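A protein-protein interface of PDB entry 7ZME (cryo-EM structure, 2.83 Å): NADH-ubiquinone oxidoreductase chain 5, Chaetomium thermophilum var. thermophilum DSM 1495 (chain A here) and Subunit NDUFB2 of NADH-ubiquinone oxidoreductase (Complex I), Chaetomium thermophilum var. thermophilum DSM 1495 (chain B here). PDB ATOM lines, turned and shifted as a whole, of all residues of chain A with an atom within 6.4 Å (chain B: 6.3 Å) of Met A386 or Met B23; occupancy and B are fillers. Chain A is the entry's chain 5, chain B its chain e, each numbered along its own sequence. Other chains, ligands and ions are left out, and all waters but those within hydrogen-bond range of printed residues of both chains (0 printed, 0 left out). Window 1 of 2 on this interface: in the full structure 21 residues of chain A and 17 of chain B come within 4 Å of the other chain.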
ATOM      1  N   ASN A 331      36.714  10.354  -5.222  1.00  0.00           N
ATOM      2  CA  ASN A 331      35.723  11.450  -5.306  1.00  0.00           C
ATOM      3  C   ASN A 331      36.443  12.743  -5.678  1.00  0.00           C
ATOM      4  O   ASN A 331      35.896  13.496  -6.479  1.00  0.00           O
ATOM      5  CB  ASN A 331      34.935  11.590  -4.008  1.00  0.00           C
ATOM      6  CG  ASN A 331      33.923  10.495  -3.769  1.00  0.00           C
ATOM      7  OD1 ASN A 331      33.154  10.566  -2.818  1.00  0.00           O
ATOM      8  ND2 ASN A 331      33.899   9.492  -4.628  1.00  0.00           N
ATOM      9  N   SER A 371      28.261  27.400 -13.495  1.00  0.00           N
ATOM     10  CA  SER A 371      27.437  26.406 -12.817  1.00  0.00           C
ATOM     11  C   SER A 371      28.236  25.155 -12.479  1.00  0.00           C
ATOM     12  O   SER A 371      28.127  24.627 -11.368  1.00  0.00           O
ATOM     13  CB  SER A 371      26.227  26.057 -13.683  1.00  0.00           C
ATOM     14  OG  SER A 371      25.408  25.086 -13.062  1.00  0.00           O
ATOM     15  N   LEU A 374      30.715  25.915  -9.783  1.00  0.00           N
ATOM     16  CA  LEU A 374      30.032  26.015  -8.497  1.00  0.00           C
ATOM     17  C   LEU A 374      29.733  24.635  -7.928  1.00  0.00           C
ATOM     18  O   LEU A 374      29.905  24.402  -6.727  1.00  0.00           O
ATOM     19  CB  LEU A 374      28.747  26.827  -8.650  1.00  0.00           C
ATOM     20  CG  LEU A 374      27.762  26.838  -7.478  1.00  0.00           C
ATOM     21  CD1 LEU A 374      28.363  27.506  -6.257  1.00  0.00           C
ATOM     22  CD2 LEU A 374      26.472  27.528  -7.878  1.00  0.00           C
ATOM     23  N   ILE A 375      29.288  23.708  -8.776  1.00  0.00           N
ATOM     24  CA  ILE A 375      29.068  22.335  -8.331  1.00  0.00           C
ATOM     25  C   ILE A 375      30.375  21.720  -7.852  1.00  0.00           C
ATOM     26  O   ILE A 375      30.430  21.063  -6.807  1.00  0.00           O
ATOM     27  CB  ILE A 375      28.431  21.502  -9.456  1.00  0.00           C
ATOM     28  CG1 ILE A 375      27.063  22.067  -9.832  1.00  0.00           C
ATOM     29  CG2 ILE A 375      28.331  20.046  -9.044  1.00  0.00           C
ATOM     30  CD1 ILE A 375      26.629  21.726 -11.225  1.00  0.00           C
ATOM     31  N   ALA A 376      31.451  21.929  -8.611  1.00  0.00           N
ATOM     32  CA  ALA A 376      32.752  21.411  -8.211  1.00  0.00           C
ATOM     33  C   ALA A 376      33.241  22.042  -6.915  1.00  0.00           C
ATOM     34  O   ALA A 376      33.949  21.392  -6.140  1.00  0.00           O
ATOM     35  CB  ALA A 376      33.767  21.638  -9.328  1.00  0.00           C
ATOM     36  N   SER A 377      32.877  23.300  -6.662  1.00  0.00           N
ATOM     37  CA  SER A 377      33.361  23.986  -5.470  1.00  0.00           C
ATOM     38  C   SER A 377      32.654  23.487  -4.217  1.00  0.00           C
ATOM     39  O   SER A 377      33.265  23.405  -3.146  1.00  0.00           O
ATOM     40  CB  SER A 377      33.172  25.491  -5.628  1.00  0.00           C
ATOM     41  OG  SER A 377      33.917  25.977  -6.729  1.00  0.00           O
ATOM     42  N   LEU A 378      31.366  23.161  -4.328  1.00  0.00           N
ATOM     43  CA  LEU A 378      30.636  22.657  -3.170  1.00  0.00           C
ATOM     44  C   LEU A 378      31.098  21.258  -2.793  1.00  0.00           C
ATOM     45  O   LEU A 378      31.195  20.932  -1.604  1.00  0.00           O
ATOM     46  CB  LEU A 378      29.134  22.685  -3.441  1.00  0.00           C
ATOM     47  CG  LEU A 378      28.534  24.083  -3.588  1.00  0.00           C
ATOM     48  CD1 LEU A 378      27.076  24.012  -3.987  1.00  0.00           C
ATOM     49  CD2 LEU A 378      28.699  24.860  -2.295  1.00  0.00           C
ATOM     50  N   SER A 379      31.443  20.460  -3.799  1.00  0.00           N
ATOM     51  CA  SER A 379      31.967  19.108  -3.505  1.00  0.00           C
ATOM     52  C   SER A 379      33.354  19.221  -2.856  1.00  0.00           C
ATOM     53  O   SER A 379      33.626  18.467  -1.925  1.00  0.00           O
ATOM     54  CB  SER A 379      31.924  18.243  -4.724  1.00  0.00           C
ATOM     55  OG  SER A 379      32.188  19.006  -5.885  1.00  0.00           O
ATOM     56  N   ALA A 382      32.981  20.212   0.602  1.00  0.00           N
ATOM     57  CA  ALA A 382      32.149  19.217   1.275  1.00  0.00           C
ATOM     58  C   ALA A 382      30.837  19.827   1.765  1.00  0.00           C
ATOM     59  O   ALA A 382      30.452  19.685   2.926  1.00  0.00           O
ATOM     60  CB  ALA A 382      32.906  18.543   2.420  1.00  0.00           C
ATOM     61  N   PHE A 383      30.154  20.522   0.864  1.00  0.00           N
ATOM     62  CA  PHE A 383      28.774  20.897   1.122  1.00  0.00           C
ATOM     63  C   PHE A 383      27.938  19.627   1.248  1.00  0.00           C
ATOM     64  O   PHE A 383      28.131  18.684   0.474  1.00  0.00           O
ATOM     65  CB  PHE A 383      28.239  21.777  -0.007  1.00  0.00           C
ATOM     66  CG  PHE A 383      27.014  22.559   0.360  1.00  0.00           C
ATOM     67  CD1 PHE A 383      27.122  23.773   1.010  1.00  0.00           C
ATOM     68  CD2 PHE A 383      25.755  22.081   0.049  1.00  0.00           C
ATOM     69  CE1 PHE A 383      25.997  24.495   1.348  1.00  0.00           C
ATOM     70  CE2 PHE A 383      24.627  22.797   0.383  1.00  0.00           C
ATOM     71  CZ  PHE A 383      24.747  24.007   1.033  1.00  0.00           C
ATOM     72  N   PRO A 384      27.001  19.571   2.194  1.00  0.00           N
ATOM     73  CA  PRO A 384      26.331  18.300   2.488  1.00  0.00           C
ATOM     74  C   PRO A 384      25.645  17.704   1.268  1.00  0.00           C
ATOM     75  O   PRO A 384      25.175  18.417   0.379  1.00  0.00           O
ATOM     76  CB  PRO A 384      25.310  18.678   3.571  1.00  0.00           C
ATOM     77  CG  PRO A 384      25.233  20.179   3.539  1.00  0.00           C
ATOM     78  CD  PRO A 384      26.589  20.632   3.124  1.00  0.00           C
ATOM     79  N   PHE A 385      25.642  16.371   1.223  1.00  0.00           N
ATOM     80  CA  PHE A 385      24.902  15.572   0.252  1.00  0.00           C
ATOM     81  C   PHE A 385      25.494  15.647  -1.148  1.00  0.00           C
ATOM     82  O   PHE A 385      24.805  15.364  -2.132  1.00  0.00           O
ATOM     83  CB  PHE A 385      23.429  15.981   0.243  1.00  0.00           C
ATOM     84  CG  PHE A 385      22.810  15.973   1.602  1.00  0.00           C
ATOM     85  CD1 PHE A 385      23.203  15.043   2.546  1.00  0.00           C
ATOM     86  CD2 PHE A 385      21.886  16.931   1.961  1.00  0.00           C
ATOM     87  CE1 PHE A 385      22.653  15.041   3.804  1.00  0.00           C
ATOM     88  CE2 PHE A 385      21.343  16.937   3.222  1.00  0.00           C
ATOM     89  CZ  PHE A 385      21.722  15.989   4.142  1.00  0.00           C
ATOM     90  N   MET A 386      26.761  16.018  -1.257  1.00  0.00           N
ATOM     91  CA  MET A 386      27.459  16.080  -2.527  1.00  0.00           C
ATOM     92  C   MET A 386      28.577  15.048  -2.513  1.00  0.00           C
ATOM     93  O   MET A 386      28.928  14.500  -1.466  1.00  0.00           O
ATOM     94  CB  MET A 386      28.001  17.490  -2.785  1.00  0.00           C
ATOM     95  CG  MET A 386      26.900  18.509  -3.056  1.00  0.00           C
ATOM     96  SD  MET A 386      26.443  18.675  -4.791  1.00  0.00           S
ATOM     97  CE  MET A 386      27.946  19.370  -5.457  1.00  0.00           C
ATOM     98  N   THR A 387      29.128  14.775  -3.698  1.00  0.00           N
ATOM     99  CA  THR A 387      30.108  13.700  -3.828  1.00  0.00           C
ATOM    100  C   THR A 387      31.275  13.891  -2.866  1.00  0.00           C
ATOM    101  O   THR A 387      31.623  12.981  -2.107  1.00  0.00           O
ATOM    102  CB  THR A 387      30.608  13.618  -5.267  1.00  0.00           C
ATOM    103  OG1 THR A 387      29.576  13.076  -6.100  1.00  0.00           O
ATOM    104  CG2 THR A 387      31.831  12.732  -5.349  1.00  0.00           C
ATOM    105  N   GLY A 388      31.878  15.080  -2.866  1.00  0.00           N
ATOM    106  CA  GLY A 388      33.005  15.339  -1.989  1.00  0.00           C
ATOM    107  C   GLY A 388      32.648  15.374  -0.520  1.00  0.00           C
ATOM    108  O   GLY A 388      33.531  15.196   0.325  1.00  0.00           O
ATOM    109  N   PHE A 389      31.372  15.601  -0.198  1.00  0.00           N
ATOM    110  CA  PHE A 389      30.939  15.639   1.196  1.00  0.00           C
ATOM    111  C   PHE A 389      31.134  14.293   1.879  1.00  0.00           C
ATOM    112  O   PHE A 389      31.700  14.217   2.973  1.00  0.00           O
ATOM    113  CB  PHE A 389      29.475  16.067   1.264  1.00  0.00           C
ATOM    114  CG  PHE A 389      28.795  15.723   2.560  1.00  0.00           C
ATOM    115  CD1 PHE A 389      29.106  16.403   3.723  1.00  0.00           C
ATOM    116  CD2 PHE A 389      27.834  14.731   2.608  1.00  0.00           C
ATOM    117  CE1 PHE A 389      28.477  16.091   4.910  1.00  0.00           C
ATOM    118  CE2 PHE A 389      27.202  14.417   3.787  1.00  0.00           C
ATOM    119  CZ  PHE A 389      27.525  15.096   4.942  1.00  0.00           C
ATOM    120  N   TYR A 390      30.671  13.215   1.242  1.00  0.00           N
ATOM    121  CA  TYR A 390      30.703  11.900   1.872  1.00  0.00           C
ATOM    122  C   TYR A 390      32.118  11.411   2.141  1.00  0.00           C
ATOM    123  O   TYR A 390      32.313  10.578   3.033  1.00  0.00           O
ATOM    124  CB  TYR A 390      29.963  10.881   1.001  1.00  0.00           C
ATOM    125  CG  TYR A 390      28.466  11.078   0.965  1.00  0.00           C
ATOM    126  CD1 TYR A 390      27.898  12.080   0.194  1.00  0.00           C
ATOM    127  CD2 TYR A 390      27.622  10.271   1.709  1.00  0.00           C
ATOM    128  CE1 TYR A 390      26.534  12.269   0.163  1.00  0.00           C
ATOM    129  CE2 TYR A 390      26.257  10.455   1.683  1.00  0.00           C
ATOM    130  CZ  TYR A 390      25.720  11.456   0.908  1.00  0.00           C
ATOM    131  OH  TYR A 390      24.360  11.644   0.877  1.00  0.00           O
ATOM    132  N   SER A 391      33.108  11.910   1.402  1.00  0.00           N
ATOM    133  CA  SER A 391      34.470  11.394   1.496  1.00  0.00           C
ATOM    134  C   SER A 391      35.321  12.178   2.489  1.00  0.00           C
ATOM    135  O   SER A 391      35.802  11.618   3.477  1.00  0.00           O
ATOM    136  CB  SER A 391      35.130  11.413   0.114  1.00  0.00           C
ATOM    137  OG  SER A 391      34.624  10.377  -0.702  1.00  0.00           O
ATOM    138  N   ALA A 478      30.040  16.944 -13.998  1.00  0.00           N
ATOM    139  CA  ALA A 478      29.164  17.582 -13.022  1.00  0.00           C
ATOM    140  C   ALA A 478      28.255  16.564 -12.351  1.00  0.00           C
ATOM    141  O   ALA A 478      28.015  16.641 -11.142  1.00  0.00           O
ATOM    142  CB  ALA A 478      28.340  18.679 -13.693  1.00  0.00           C
ATOM    143  N   PHE A 480      28.848  13.456 -11.728  1.00  0.00           N
ATOM    144  CA  PHE A 480      29.615  12.720 -10.729  1.00  0.00           C
ATOM    145  C   PHE A 480      29.731  13.506  -9.430  1.00  0.00           C
ATOM    146  O   PHE A 480      29.594  12.942  -8.340  1.00  0.00           O
ATOM    147  CB  PHE A 480      31.001  12.384 -11.274  1.00  0.00           C
ATOM    148  CG  PHE A 480      31.022  11.189 -12.180  1.00  0.00           C
ATOM    149  CD1 PHE A 480      30.563  11.280 -13.478  1.00  0.00           C
ATOM    150  CD2 PHE A 480      31.502   9.975 -11.729  1.00  0.00           C
ATOM    151  CE1 PHE A 480      30.583  10.186 -14.310  1.00  0.00           C
ATOM    152  CE2 PHE A 480      31.524   8.877 -12.557  1.00  0.00           C
ATOM    153  CZ  PHE A 480      31.064   8.984 -13.851  1.00  0.00           C
ATOM    154  N   SER A 481      29.975  14.811  -9.523  1.00  0.00           N
ATOM    155  CA  SER A 481      30.191  15.611  -8.326  1.00  0.00           C
ATOM    156  C   SER A 481      28.911  15.872  -7.544  1.00  0.00           C
ATOM    157  O   SER A 481      28.989  16.395  -6.428  1.00  0.00           O
ATOM    158  CB  SER A 481      30.854  16.933  -8.699  1.00  0.00           C
ATOM    159  OG  SER A 481      31.943  16.716  -9.576  1.00  0.00           O
ATOM    160  N   ILE A 482      27.747  15.538  -8.092  1.00  0.00           N
ATOM    161  CA  ILE A 482      26.487  15.670  -7.377  1.00  0.00           C
ATOM    162  C   ILE A 482      26.040  14.343  -6.775  1.00  0.00           C
ATOM    163  O   ILE A 482      25.485  14.320  -5.678  1.00  0.00           O
ATOM    164  CB  ILE A 482      25.396  16.245  -8.306  1.00  0.00           C
ATOM    165  CG1 ILE A 482      25.886  17.509  -9.000  1.00  0.00           C
ATOM    166  CG2 ILE A 482      24.124  16.546  -7.527  1.00  0.00           C
ATOM    167  CD1 ILE A 482      24.886  18.103  -9.947  1.00  0.00           C
ATOM    168  N   PHE A 483      26.285  13.230  -7.464  1.00  0.00           N
ATOM    169  CA  PHE A 483      25.666  11.963  -7.102  1.00  0.00           C
ATOM    170  C   PHE A 483      26.634  10.819  -6.839  1.00  0.00           C
ATOM    171  O   PHE A 483      26.274   9.906  -6.097  1.00  0.00           O
ATOM    172  CB  PHE A 483      24.694  11.510  -8.203  1.00  0.00           C
ATOM    173  CG  PHE A 483      23.693  12.552  -8.593  1.00  0.00           C
ATOM    174  CD1 PHE A 483      22.602  12.817  -7.786  1.00  0.00           C
ATOM    175  CD2 PHE A 483      23.842  13.267  -9.769  1.00  0.00           C
ATOM    176  CE1 PHE A 483      21.681  13.773  -8.140  1.00  0.00           C
ATOM    177  CE2 PHE A 483      22.922  14.226 -10.129  1.00  0.00           C
ATOM    178  CZ  PHE A 483      21.839  14.479  -9.315  1.00  0.00           C
ATOM    179  N   GLY A 485      29.331  10.136  -5.113  1.00  0.00           N
ATOM    180  CA  GLY A 485      29.696   9.773  -3.754  1.00  0.00           C
ATOM    181  C   GLY A 485      28.590   9.035  -3.024  1.00  0.00           C
ATOM    182  O   GLY A 485      28.847   8.072  -2.299  1.00  0.00           O
ATOM    183  N   PHE A 486      27.346   9.473  -3.210  1.00  0.00           N
ATOM    184  CA  PHE A 486      26.225   8.813  -2.551  1.00  0.00           C
ATOM    185  C   PHE A 486      26.026   7.393  -3.063  1.00  0.00           C
ATOM    186  O   PHE A 486      25.736   6.482  -2.281  1.00  0.00           O
ATOM    187  CB  PHE A 486      24.953   9.636  -2.739  1.00  0.00           C
ATOM    188  CG  PHE A 486      23.724   8.985  -2.182  1.00  0.00           C
ATOM    189  CD1 PHE A 486      23.362   9.188  -0.866  1.00  0.00           C
ATOM    190  CD2 PHE A 486      22.926   8.180  -2.976  1.00  0.00           C
ATOM    191  CE1 PHE A 486      22.235   8.596  -0.350  1.00  0.00           C
ATOM    192  CE2 PHE A 486      21.802   7.586  -2.465  1.00  0.00           C
ATOM    193  CZ  PHE A 486      21.452   7.794  -1.150  1.00  0.00           C
ATOM    194  N   GLY B  18      19.962  23.448 -15.578  1.00  0.00           N
ATOM    195  CA  GLY B  18      19.610  22.071 -15.266  1.00  0.00           C
ATOM    196  C   GLY B  18      20.544  21.447 -14.248  1.00  0.00           C
ATOM    197  O   GLY B  18      20.103  20.788 -13.303  1.00  0.00           O
ATOM    198  N   LEU B  19      21.850  21.646 -14.426  1.00  0.00           N
ATOM    199  CA  LEU B  19      22.811  21.119 -13.464  1.00  0.00           C
ATOM    200  C   LEU B  19      22.640  21.774 -12.102  1.00  0.00           C
ATOM    201  O   LEU B  19      22.694  21.099 -11.069  1.00  0.00           O
ATOM    202  CB  LEU B  19      24.231  21.318 -13.983  1.00  0.00           C
ATOM    203  CG  LEU B  19      24.572  20.500 -15.223  1.00  0.00           C
ATOM    204  CD1 LEU B  19      25.967  20.831 -15.719  1.00  0.00           C
ATOM    205  CD2 LEU B  19      24.449  19.023 -14.914  1.00  0.00           C
ATOM    206  N   GLY B  20      22.435  23.092 -12.079  1.00  0.00           N
ATOM    207  CA  GLY B  20      22.180  23.765 -10.818  1.00  0.00           C
ATOM    208  C   GLY B  20      20.864  23.341 -10.196  1.00  0.00           C
ATOM    209  O   GLY B  20      20.777  23.147  -8.981  1.00  0.00           O
ATOM    210  N   ALA B  21      19.822  23.203 -11.017  1.00  0.00           N
ATOM    211  CA  ALA B  21      18.545  22.718 -10.506  1.00  0.00           C
ATOM    212  C   ALA B  21      18.654  21.278 -10.033  1.00  0.00           C
ATOM    213  O   ALA B  21      18.127  20.927  -8.973  1.00  0.00           O
ATOM    214  CB  ALA B  21      17.462  22.852 -11.576  1.00  0.00           C
ATOM    215  N   SER B  22      19.332  20.427 -10.807  1.00  0.00           N
ATOM    216  CA  SER B  22      19.501  19.038 -10.393  1.00  0.00           C
ATOM    217  C   SER B  22      20.315  18.948  -9.113  1.00  0.00           C
ATOM    218  O   SER B  22      20.008  18.138  -8.230  1.00  0.00           O
ATOM    219  CB  SER B  22      20.167  18.226 -11.503  1.00  0.00           C
ATOM    220  OG  SER B  22      21.495  18.665 -11.725  1.00  0.00           O
ATOM    221  N   MET B  23      21.361  19.767  -8.996  1.00  0.00           N
ATOM    222  CA  MET B  23      22.160  19.769  -7.778  1.00  0.00           C
ATOM    223  C   MET B  23      21.306  20.135  -6.576  1.00  0.00           C
ATOM    224  O   MET B  23      21.136  19.330  -5.655  1.00  0.00           O
ATOM    225  CB  MET B  23      23.336  20.734  -7.906  1.00  0.00           C
ATOM    226  CG  MET B  23      24.106  20.901  -6.609  1.00  0.00           C
ATOM    227  SD  MET B  23      25.432  22.112  -6.684  1.00  0.00           S
ATOM    228  CE  MET B  23      24.495  23.625  -6.841  1.00  0.00           C
ATOM    229  N   TRP B  24      20.731  21.340  -6.584  1.00  0.00           N
ATOM    230  CA  TRP B  24      20.007  21.817  -5.410  1.00  0.00           C
ATOM    231  C   TRP B  24      18.844  20.905  -5.064  1.00  0.00           C
ATOM    232  O   TRP B  24      18.689  20.515  -3.903  1.00  0.00           O
ATOM    233  CB  TRP B  24      19.529  23.250  -5.619  1.00  0.00           C
ATOM    234  CG  TRP B  24      20.644  24.237  -5.542  1.00  0.00           C
ATOM    235  CD1 TRP B  24      21.075  25.062  -6.533  1.00  0.00           C
ATOM    236  CD2 TRP B  24      21.484  24.489  -4.412  1.00  0.00           C
ATOM    237  NE1 TRP B  24      22.128  25.819  -6.089  1.00  0.00           N
ATOM    238  CE2 TRP B  24      22.399  25.486  -4.789  1.00  0.00           C
ATOM    239  CE3 TRP B  24      21.548  23.971  -3.117  1.00  0.00           C
ATOM    240  CZ2 TRP B  24      23.368  25.975  -3.920  1.00  0.00           C
ATOM    241  CZ3 TRP B  24      22.508  24.457  -2.256  1.00  0.00           C
ATOM    242  CH2 TRP B  24      23.407  25.449  -2.660  1.00  0.00           C
ATOM    243  N   PHE B  25      18.051  20.506  -6.063  1.00  0.00           N
ATOM    244  CA  PHE B  25      16.931  19.611  -5.790  1.00  0.00           C
ATOM    245  C   PHE B  25      17.394  18.343  -5.092  1.00  0.00           C
ATOM    246  O   PHE B  25      16.634  17.742  -4.327  1.00  0.00           O
ATOM    247  CB  PHE B  25      16.200  19.265  -7.084  1.00  0.00           C
ATOM    248  CG  PHE B  25      15.094  18.265  -6.904  1.00  0.00           C
ATOM    249  CD1 PHE B  25      13.908  18.629  -6.290  1.00  0.00           C
ATOM    250  CD2 PHE B  25      15.244  16.961  -7.341  1.00  0.00           C
ATOM    251  CE1 PHE B  25      12.891  17.712  -6.120  1.00  0.00           C
ATOM    252  CE2 PHE B  25      14.231  16.039  -7.172  1.00  0.00           C
ATOM    253  CZ  PHE B  25      13.053  16.415  -6.562  1.00  0.00           C
ATOM    254  N   TRP B  26      18.637  17.928  -5.340  1.00  0.00           N
ATOM    255  CA  TRP B  26      19.187  16.761  -4.662  1.00  0.00           C
ATOM    256  C   TRP B  26      19.446  17.040  -3.185  1.00  0.00           C
ATOM    257  O   TRP B  26      19.165  16.185  -2.339  1.00  0.00           O
ATOM    258  CB  TRP B  26      20.461  16.310  -5.375  1.00  0.00           C
ATOM    259  CG  TRP B  26      21.256  15.274  -4.650  1.00  0.00           C
ATOM    260  CD1 TRP B  26      22.385  15.480  -3.920  1.00  0.00           C
ATOM    261  CD2 TRP B  26      20.993  13.869  -4.594  1.00  0.00           C
ATOM    262  NE1 TRP B  26      22.842  14.295  -3.407  1.00  0.00           N
ATOM    263  CE2 TRP B  26      22.003  13.288  -3.805  1.00  0.00           C
ATOM    264  CE3 TRP B  26      20.001  13.046  -5.130  1.00  0.00           C
ATOM    265  CZ2 TRP B  26      22.049  11.924  -3.540  1.00  0.00           C
ATOM    266  CZ3 TRP B  26      20.049  11.694  -4.865  1.00  0.00           C
ATOM    267  CH2 TRP B  26      21.067  11.145  -4.078  1.00  0.00           C
ATOM    268  N   ILE B  27      19.975  18.222  -2.845  1.00  0.00           N
ATOM    269  CA  ILE B  27      20.279  18.507  -1.442  1.00  0.00           C
ATOM    270  C   ILE B  27      19.007  18.542  -0.600  1.00  0.00           C
ATOM    271  O   ILE B  27      18.966  17.977   0.499  1.00  0.00           O
ATOM    272  CB  ILE B  27      21.103  19.800  -1.282  1.00  0.00           C
ATOM    273  CG1 ILE B  27      22.429  19.725  -2.043  1.00  0.00           C
ATOM    274  CG2 ILE B  27      21.367  20.095   0.182  1.00  0.00           C
ATOM    275  CD1 ILE B  27      22.493  20.523  -3.291  1.00  0.00           C
ATOM    276  N   PHE B  28      17.952  19.204  -1.086  1.00  0.00           N
ATOM    277  CA  PHE B  28      16.690  19.148  -0.352  1.00  0.00           C
ATOM    278  C   PHE B  28      16.172  17.720  -0.251  1.00  0.00           C
ATOM    279  O   PHE B  28      15.718  17.294   0.818  1.00  0.00           O
ATOM    280  CB  PHE B  28      15.620  20.052  -0.978  1.00  0.00           C
ATOM    281  CG  PHE B  28      16.045  21.481  -1.179  1.00  0.00           C
ATOM    282  CD1 PHE B  28      16.833  21.855  -2.246  1.00  0.00           C
ATOM    283  CD2 PHE B  28      15.632  22.460  -0.289  1.00  0.00           C
ATOM    284  CE1 PHE B  28      17.211  23.171  -2.425  1.00  0.00           C
ATOM    285  CE2 PHE B  28      16.004  23.779  -0.459  1.00  0.00           C
ATOM    286  CZ  PHE B  28      16.795  24.135  -1.529  1.00  0.00           C
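The backbone carbonyl oxygen (O) of Gly B18 is in hydrogen-bond range of the side-chain hydroxyl (OG) of Ser B22, at 3.0 Å. The backbone carbonyl oxygen (O) of Leu A378 is in hydrogen-bond range of the backbone NH (N) of Phe A383, at 2.7 Å. O of Leu B19 lies within hydrogen-bond range of OG of Ser B22, at 2.8 Å. The side-chain hydroxyl (OG) of Ser A379 lies within hydrogen-bond range of the backbone carbonyl oxygen (O) of Ile A375 (2.9 Å).
Of the 11 printed residues of chain B, 7 touch a printed residue of chain A. Along chain B the printed residues that touch a printed residue of chain A span positions 19 to 27.
The backbone carbonyl oxygen (O) of Phe A385 is in hydrogen-bond range of the indole nitrogen (NE1) of Trp B26 (2.6 Å). The indole nitrogen (NE1) of Trp B26 lies within hydrogen-bond range of the backbone carbonyl oxygen (O) of Ile A482 (3.5 Å).
Leu B19 touches Ile A375. Met B23 touches Ile A375 (SD to CG1, 3.5 Å). Leu A378 touches Met B23. Phe A383 touches Trp B24 (CE2 to CZ3, 3.8 Å). Phe A385 touches Ile B27. Leu B19 touches Ala A478. Ile A482 touches Ser B22 (CD1 to OG, 3.9 Å). CD1 of Ile A482 touches CB of Met B23 (3.7 Å). Phe A483 touches Trp B26 (CE1 to CE3, 3.5 Å). Trp B26 touches Phe A486 (CZ2 to CG, 3.6 Å).
Of the printed residues of chain B, Phe A385 touches Trp B26 and Ile B27. Met A386 touches just one residue of chain B: Met B23. Phe A389 touches none of the printed residues of chain B. Of the printed residues of chain B, Ala A478 touches Leu B19. Of the printed residues of chain A, Ser B22 touches Ile A482. Of chain A, only Ile A375, Leu A378, Met A386 and Ile A482 come within 4 Å of Met B23. Printed residues of chain A within 4 Å of Ile B27: Pro A384 and Phe A385. The nearest residue of chain A that does not touch Met B23 is Leu A374 (4.5 Å).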
